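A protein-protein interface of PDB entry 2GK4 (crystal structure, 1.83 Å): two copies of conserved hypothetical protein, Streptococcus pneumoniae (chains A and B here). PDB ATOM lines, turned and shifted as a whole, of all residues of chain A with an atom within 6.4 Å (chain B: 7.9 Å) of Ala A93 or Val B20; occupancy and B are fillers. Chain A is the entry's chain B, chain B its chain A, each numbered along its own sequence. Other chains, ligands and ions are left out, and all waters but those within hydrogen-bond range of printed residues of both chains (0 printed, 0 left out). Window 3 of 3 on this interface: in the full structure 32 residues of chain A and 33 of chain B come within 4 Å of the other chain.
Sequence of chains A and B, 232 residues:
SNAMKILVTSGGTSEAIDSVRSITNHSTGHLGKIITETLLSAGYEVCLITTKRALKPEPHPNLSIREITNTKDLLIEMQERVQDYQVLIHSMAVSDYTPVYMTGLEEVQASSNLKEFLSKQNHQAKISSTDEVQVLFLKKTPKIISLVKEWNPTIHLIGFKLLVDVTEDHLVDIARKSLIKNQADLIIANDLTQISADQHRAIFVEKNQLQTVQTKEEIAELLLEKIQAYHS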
ATOM      1  N   THR A   9      16.413   5.639  34.347  1.00  0.00           N
ATOM      2  CA  THR A   9      15.196   4.875  34.000  1.00  0.00           C
ATOM      3  C   THR A   9      14.835   5.207  32.560  1.00  0.00           C
ATOM      4  O   THR A   9      15.095   6.340  32.084  1.00  0.00           O
ATOM      5  CB  THR A   9      13.986   5.209  34.910  1.00  0.00           C
ATOM      6  OG1 THR A   9      13.543   6.527  34.591  1.00  0.00           O
ATOM      7  CG2 THR A   9      14.361   5.172  36.415  1.00  0.00           C
ATOM      8  N   SER A  10      14.227   4.248  31.868  1.00  0.00           N
ATOM      9  CA  SER A  10      13.774   4.476  30.500  1.00  0.00           C
ATOM     10  C   SER A  10      12.658   3.511  30.123  1.00  0.00           C
ATOM     11  O   SER A  10      12.451   2.520  30.814  1.00  0.00           O
ATOM     12  CB  SER A  10      14.938   4.330  29.510  1.00  0.00           C
ATOM     13  OG  SER A  10      15.289   2.966  29.325  1.00  0.00           O
ATOM     14  N   GLY A  11      11.991   3.763  29.003  1.00  0.00           N
ATOM     15  CA  GLY A  11      10.892   2.868  28.569  1.00  0.00           C
ATOM     16  C   GLY A  11       9.546   3.325  29.100  1.00  0.00           C
ATOM     17  O   GLY A  11       9.345   4.514  29.376  1.00  0.00           O
ATOM     18  N   GLY A  12       8.596   2.398  29.221  1.00  0.00           N
ATOM     19  CA  GLY A  12       7.266   2.771  29.674  1.00  0.00           C
ATOM     20  C   GLY A  12       6.578   1.643  30.431  1.00  0.00           C
ATOM     21  O   GLY A  12       6.640   0.495  30.018  1.00  0.00           O
ATOM     22  N   THR A  13       5.939   2.005  31.536  1.00  0.00           N
ATOM     23  CA  THR A  13       5.310   1.071  32.457  1.00  0.00           C
ATOM     24  C   THR A  13       3.876   0.760  31.987  1.00  0.00           C
ATOM     25  O   THR A  13       3.328   1.437  31.094  1.00  0.00           O
ATOM     26  CB  THR A  13       5.240   1.646  33.913  1.00  0.00           C
ATOM     27  OG1 THR A  13       4.649   2.951  33.914  1.00  0.00           O
ATOM     28  CG2 THR A  13       6.593   1.706  34.576  1.00  0.00           C
ATOM     29  N   SER A  14       3.301  -0.290  32.568  1.00  0.00           N
ATOM     30  CA  SER A  14       1.900  -0.642  32.345  1.00  0.00           C
ATOM     31  C   SER A  14       1.223  -0.753  33.703  1.00  0.00           C
ATOM     32  O   SER A  14       1.887  -0.980  34.730  1.00  0.00           O
ATOM     33  CB  SER A  14       1.767  -1.985  31.612  1.00  0.00           C
ATOM     34  OG  SER A  14       2.601  -2.064  30.470  1.00  0.00           O
ATOM     35  N   THR A  24      -1.175   1.261  29.147  1.00  0.00           N
ATOM     36  CA  THR A  24       0.227   1.059  28.801  1.00  0.00           C
ATOM     37  C   THR A  24       0.841   2.393  28.366  1.00  0.00           C
ATOM     38  O   THR A  24       0.152   3.235  27.817  1.00  0.00           O
ATOM     39  CB  THR A  24       0.382   0.005  27.679  1.00  0.00           C
ATOM     40  OG1 THR A  24      -0.384   0.422  26.531  1.00  0.00           O
ATOM     41  CG2 THR A  24      -0.169  -1.372  28.159  1.00  0.00           C
ATOM     42  N   ASN A  25       2.138   2.569  28.612  1.00  0.00           N
ATOM     43  CA  ASN A  25       2.875   3.771  28.206  1.00  0.00           C
ATOM     44  C   ASN A  25       3.943   3.392  27.196  1.00  0.00           C
ATOM     45  O   ASN A  25       4.708   2.469  27.439  1.00  0.00           O
ATOM     46  CB  ASN A  25       3.543   4.402  29.427  1.00  0.00           C
ATOM     47  CG  ASN A  25       2.538   4.875  30.439  1.00  0.00           C
ATOM     48  OD1 ASN A  25       2.198   4.157  31.380  1.00  0.00           O
ATOM     49  ND2 ASN A  25       2.022   6.064  30.233  1.00  0.00           N
ATOM     50  N   HIS A  26       3.984   4.099  26.069  1.00  0.00           N
ATOM     51  CA  HIS A  26       4.982   3.847  25.040  1.00  0.00           C
ATOM     52  C   HIS A  26       6.101   4.886  25.095  1.00  0.00           C
ATOM     53  O   HIS A  26       5.855   6.115  25.091  1.00  0.00           O
ATOM     54  CB  HIS A  26       4.346   3.772  23.636  1.00  0.00           C
ATOM     55  CG  HIS A  26       5.347   3.681  22.516  1.00  0.00           C
ATOM     56  ND1 HIS A  26       6.043   2.525  22.222  1.00  0.00           N
ATOM     57  CD2 HIS A  26       5.762   4.606  21.617  1.00  0.00           C
ATOM     58  CE1 HIS A  26       6.846   2.743  21.194  1.00  0.00           C
ATOM     59  NE2 HIS A  26       6.698   4.000  20.812  1.00  0.00           N
ATOM     60  N   SER A  27       7.320   4.366  25.224  1.00  0.00           N
ATOM     61  CA  SER A  27       8.536   5.123  24.997  1.00  0.00           C
ATOM     62  C   SER A  27       9.576   4.111  24.528  1.00  0.00           C
ATOM     63  O   SER A  27       9.734   3.043  25.132  1.00  0.00           O
ATOM     64  CB  SER A  27       9.025   5.799  26.277  1.00  0.00           C
ATOM     65  OG  SER A  27      10.210   6.555  26.001  1.00  0.00           O
ATOM     66  N   HIS A  90      15.566  10.229  35.475  1.00  0.00           N
ATOM     67  CA  HIS A  90      14.296   9.507  35.335  1.00  0.00           C
ATOM     68  C   HIS A  90      13.650   9.863  34.007  1.00  0.00           C
ATOM     69  O   HIS A  90      13.012  10.924  33.886  1.00  0.00           O
ATOM     70  CB  HIS A  90      13.389   9.845  36.530  1.00  0.00           C
ATOM     71  CG  HIS A  90      12.028   9.216  36.471  1.00  0.00           C
ATOM     72  ND1 HIS A  90      11.829   7.869  36.233  1.00  0.00           N
ATOM     73  CD2 HIS A  90      10.795   9.750  36.660  1.00  0.00           C
ATOM     74  CE1 HIS A  90      10.532   7.607  36.256  1.00  0.00           C
ATOM     75  NE2 HIS A  90       9.882   8.727  36.526  1.00  0.00           N
ATOM     76  N   SER A  91      13.814   8.994  33.015  1.00  0.00           N
ATOM     77  CA  SER A  91      13.237   9.237  31.688  1.00  0.00           C
ATOM     78  C   SER A  91      12.121   8.272  31.303  1.00  0.00           C
ATOM     79  O   SER A  91      11.533   8.407  30.217  1.00  0.00           O
ATOM     80  CB  SER A  91      14.317   9.267  30.590  1.00  0.00           C
ATOM     81  OG  SER A  91      14.669   7.965  30.141  1.00  0.00           O
ATOM     82  N   MET A  92      11.863   7.282  32.155  1.00  0.00           N
ATOM     83  CA  MET A  92      10.781   6.341  31.910  1.00  0.00           C
ATOM     84  C   MET A  92       9.436   7.065  31.848  1.00  0.00           C
ATOM     85  O   MET A  92       9.188   7.990  32.649  1.00  0.00           O
ATOM     86  CB  MET A  92      10.734   5.282  33.017  1.00  0.00           C
ATOM     87  CG  MET A  92       9.765   4.149  32.749  1.00  0.00           C
ATOM     88  SD  MET A  92       9.828   2.961  34.288  1.00  0.00           S
ATOM     89  CE  MET A  92      11.340   1.783  33.723  1.00  0.00           C
ATOM     90  N   ALA A  93       8.598   6.660  30.888  1.00  0.00           N
ATOM     91  CA  ALA A  93       7.203   7.111  30.817  1.00  0.00           C
ATOM     92  C   ALA A  93       6.375   6.302  31.826  1.00  0.00           C
ATOM     93  O   ALA A  93       6.336   5.071  31.786  1.00  0.00           O
ATOM     94  CB  ALA A  93       6.649   6.935  29.423  1.00  0.00           C
ATOM     95  N   VAL A  94       5.755   7.023  32.749  1.00  0.00           N
ATOM     96  CA  VAL A  94       4.934   6.450  33.792  1.00  0.00           C
ATOM     97  C   VAL A  94       3.628   7.263  33.789  1.00  0.00           C
ATOM     98  O   VAL A  94       3.669   8.476  33.690  1.00  0.00           O
ATOM     99  CB  VAL A  94       5.644   6.593  35.155  1.00  0.00           C
ATOM    100  CG1 VAL A  94       4.780   6.060  36.268  1.00  0.00           C
ATOM    101  CG2 VAL A  94       7.002   5.875  35.140  1.00  0.00           C
ATOM    102  N   SER A  95       2.475   6.616  33.858  1.00  0.00           N
ATOM    103  CA  SER A  95       1.235   7.412  33.881  1.00  0.00           C
ATOM    104  C   SER A  95       1.085   8.117  35.229  1.00  0.00           C
ATOM    105  O   SER A  95       1.245   7.513  36.295  1.00  0.00           O
ATOM    106  CB  SER A  95      -0.011   6.585  33.523  1.00  0.00           C
ATOM    107  OG  SER A  95      -1.202   7.387  33.559  1.00  0.00           O
ATOM    108  N   LEU A 162       7.376  15.957  29.349  1.00  0.00           N
ATOM    109  CA  LEU A 162       6.978  15.943  27.939  1.00  0.00           C
ATOM    110  C   LEU A 162       5.544  16.477  27.813  1.00  0.00           C
ATOM    111  O   LEU A 162       4.616  15.904  28.383  1.00  0.00           O
ATOM    112  CB  LEU A 162       7.101  14.528  27.344  1.00  0.00           C
ATOM    113  CG  LEU A 162       6.767  14.273  25.863  1.00  0.00           C
ATOM    114  CD1 LEU A 162       7.619  15.087  24.905  1.00  0.00           C
ATOM    115  CD2 LEU A 162       6.988  12.805  25.559  1.00  0.00           C
ATOM    116  N   ALA B  16      -5.145   4.010  21.362  1.00  0.00           N
ATOM    117  CA  ALA B  16      -4.435   5.201  21.875  1.00  0.00           C
ATOM    118  C   ALA B  16      -5.350   6.148  22.643  1.00  0.00           C
ATOM    119  O   ALA B  16      -6.487   6.434  22.222  1.00  0.00           O
ATOM    120  CB  ALA B  16      -3.715   5.941  20.749  1.00  0.00           C
ATOM    121  N   ILE B  17      -4.870   6.592  23.794  1.00  0.00           N
ATOM    122  CA  ILE B  17      -5.550   7.623  24.575  1.00  0.00           C
ATOM    123  C   ILE B  17      -4.958   8.979  24.201  1.00  0.00           C
ATOM    124  O   ILE B  17      -5.677   9.958  23.940  1.00  0.00           O
ATOM    125  CB  ILE B  17      -5.391   7.378  26.091  1.00  0.00           C
ATOM    126  CG1 ILE B  17      -6.223   6.160  26.508  1.00  0.00           C
ATOM    127  CG2 ILE B  17      -5.858   8.595  26.887  1.00  0.00           C
ATOM    128  CD1 ILE B  17      -5.863   5.609  27.897  1.00  0.00           C
ATOM    129  N   ASP B  18      -3.645   9.033  24.184  1.00  0.00           N
ATOM    130  CA  ASP B  18      -2.961  10.256  23.838  1.00  0.00           C
ATOM    131  C   ASP B  18      -1.672   9.826  23.198  1.00  0.00           C
ATOM    132  O   ASP B  18      -1.567   8.692  22.705  1.00  0.00           O
ATOM    133  CB  ASP B  18      -2.744  11.133  25.084  1.00  0.00           C
ATOM    134  CG  ASP B  18      -1.945  10.422  26.184  1.00  0.00           C
ATOM    135  OD1 ASP B  18      -0.882   9.793  25.904  1.00  0.00           O
ATOM    136  OD2 ASP B  18      -2.364  10.544  27.345  1.00  0.00           O
ATOM    137  N   SER B  19      -0.670  10.704  23.215  1.00  0.00           N
ATOM    138  CA  SER B  19       0.561  10.427  22.476  1.00  0.00           C
ATOM    139  C   SER B  19       1.339   9.286  23.100  1.00  0.00           C
ATOM    140  O   SER B  19       1.973   8.498  22.386  1.00  0.00           O
ATOM    141  CB  SER B  19       1.442  11.688  22.345  1.00  0.00           C
ATOM    142  OG  SER B  19       1.852  12.209  23.605  1.00  0.00           O
ATOM    143  N   VAL B  20       1.271   9.177  24.429  1.00  0.00           N
ATOM    144  CA  VAL B  20       2.042   8.157  25.151  1.00  0.00           C
ATOM    145  C   VAL B  20       1.201   6.948  25.627  1.00  0.00           C
ATOM    146  O   VAL B  20       1.645   5.790  25.511  1.00  0.00           O
ATOM    147  CB  VAL B  20       2.864   8.816  26.310  1.00  0.00           C
ATOM    148  CG1 VAL B  20       3.563   7.765  27.162  1.00  0.00           C
ATOM    149  CG2 VAL B  20       3.916   9.783  25.706  1.00  0.00           C
ATOM    150  N   ARG B  21      -0.026   7.203  26.074  1.00  0.00           N
ATOM    151  CA  ARG B  21      -0.806   6.165  26.772  1.00  0.00           C
ATOM    152  C   ARG B  21      -1.800   5.497  25.829  1.00  0.00           C
ATOM    153  O   ARG B  21      -2.337   6.154  24.944  1.00  0.00           O
ATOM    154  CB  ARG B  21      -1.550   6.778  27.966  1.00  0.00           C
ATOM    155  CG  ARG B  21      -0.628   7.359  29.020  1.00  0.00           C
ATOM    156  CD  ARG B  21      -1.434   7.901  30.205  1.00  0.00           C
ATOM    157  NE  ARG B  21      -2.398   8.930  29.809  1.00  0.00           N
ATOM    158  CZ  ARG B  21      -3.343   9.432  30.606  1.00  0.00           C
ATOM    159  NH1 ARG B  21      -3.465   9.020  31.866  1.00  0.00           N
ATOM    160  NH2 ARG B  21      -4.160  10.370  30.141  1.00  0.00           N
ATOM    161  N   SER B  22      -2.037   4.201  26.049  1.00  0.00           N
ATOM    162  CA  SER B  22      -3.087   3.442  25.353  1.00  0.00           C
ATOM    163  C   SER B  22      -3.833   2.595  26.343  1.00  0.00           C
ATOM    164  O   SER B  22      -3.297   2.328  27.436  1.00  0.00           O
ATOM    165  CB  SER B  22      -2.413   2.512  24.346  1.00  0.00           C
ATOM    166  OG  SER B  22      -1.862   3.299  23.285  1.00  0.00           O
ATOM    167  N   ILE B  23      -5.058   2.197  26.001  1.00  0.00           N
ATOM    168  CA  ILE B  23      -5.695   1.125  26.766  1.00  0.00           C
ATOM    169  C   ILE B  23      -5.559  -0.114  25.895  1.00  0.00           C
ATOM    170  O   ILE B  23      -5.972  -0.137  24.717  1.00  0.00           O
ATOM    171  CB  ILE B  23      -7.165   1.426  27.112  1.00  0.00           C
ATOM    172  CG1 ILE B  23      -7.799   0.230  27.830  1.00  0.00           C
ATOM    173  CG2 ILE B  23      -7.981   1.879  25.865  1.00  0.00           C
ATOM    174  CD1 ILE B  23      -9.131   0.617  28.516  1.00  0.00           C
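Ala A93 touches just one residue of chain B: Val B20 (3.9 Å).
Of chain A, only Thr A24, Asn A25, His A26 and Ala A93 come within 4 Å of Val B20.
Printed residues of chain A within 4 Å of Ser B22: Thr A24.
Of the printed residues of chain B, Asn A25 touches Val B20 and Arg B21.
Printed residues of chain A within 4 Å of Arg B21: Thr A24, Asn A25 and Ser A95.
Of the printed residues of chain B, Ser A95 touches Arg B21.
Met A92 touches none of the printed residues of chain B.
Ile B23 touches none of the printed residues of chain A.
The nearest printed residue of chain B that does not touch His A26 is Arg B21 (5.1 Å).
No position is printed for both chains.
Of the 8 pairs that touch across the chains among the printed residues, none has its exchanged pair printed and touching as well.
O of Thr A24 touches O of Val B20, 3.8 Å away.
Thr A24 touches Arg B21 (O to CA, 3.3 Å).
Val B20 touches Asn A25.
Arg B21 touches Asn A25 (CG to ND2, 3.2 Å).
Ala A93 touches Val B20.
OD2 of Asp B18 lies within salt-bridge range of NE of Arg B21, at 2.9 Å.
The backbone carbonyl oxygen of Gly A11 sits at hydrogen-bond distance from the backbone NH of Ala A93 (2.7 Å).
O of Thr A13 sits close to OD1 of Asn A25 (3.0 Å).
N of Thr A13 lies within hydrogen-bond range of O of Ala A93, at 3.1 Å.
The backbone NH (N) of Val B20 lies within hydrogen-bond range of the side-chain carboxylate (OD1) of Asp B18 (2.7 Å).
N of His A26 sits at hydrogen-bond distance from O of Val B20.
The backbone carbonyl oxygen (O) of Ser B22 is in hydrogen-bond range of the backbone NH (N) of Thr A24 (2.9 Å).
The guanidinium group (NH1) of Arg B21 lies within hydrogen-bond range of the side-chain hydroxyl (OG) of Ser A95 (3.3 Å).
Of the 17 printed residues of chain A, 5 touch a printed residue of chain B.
Along chain A the printed residues that touch a printed residue of chain B span positions 24 to 95.
Among the printed residues, no Asp or Glu carboxylate lies within 4 Å of a Lys or Arg side-chain nitrogen of the other chain.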
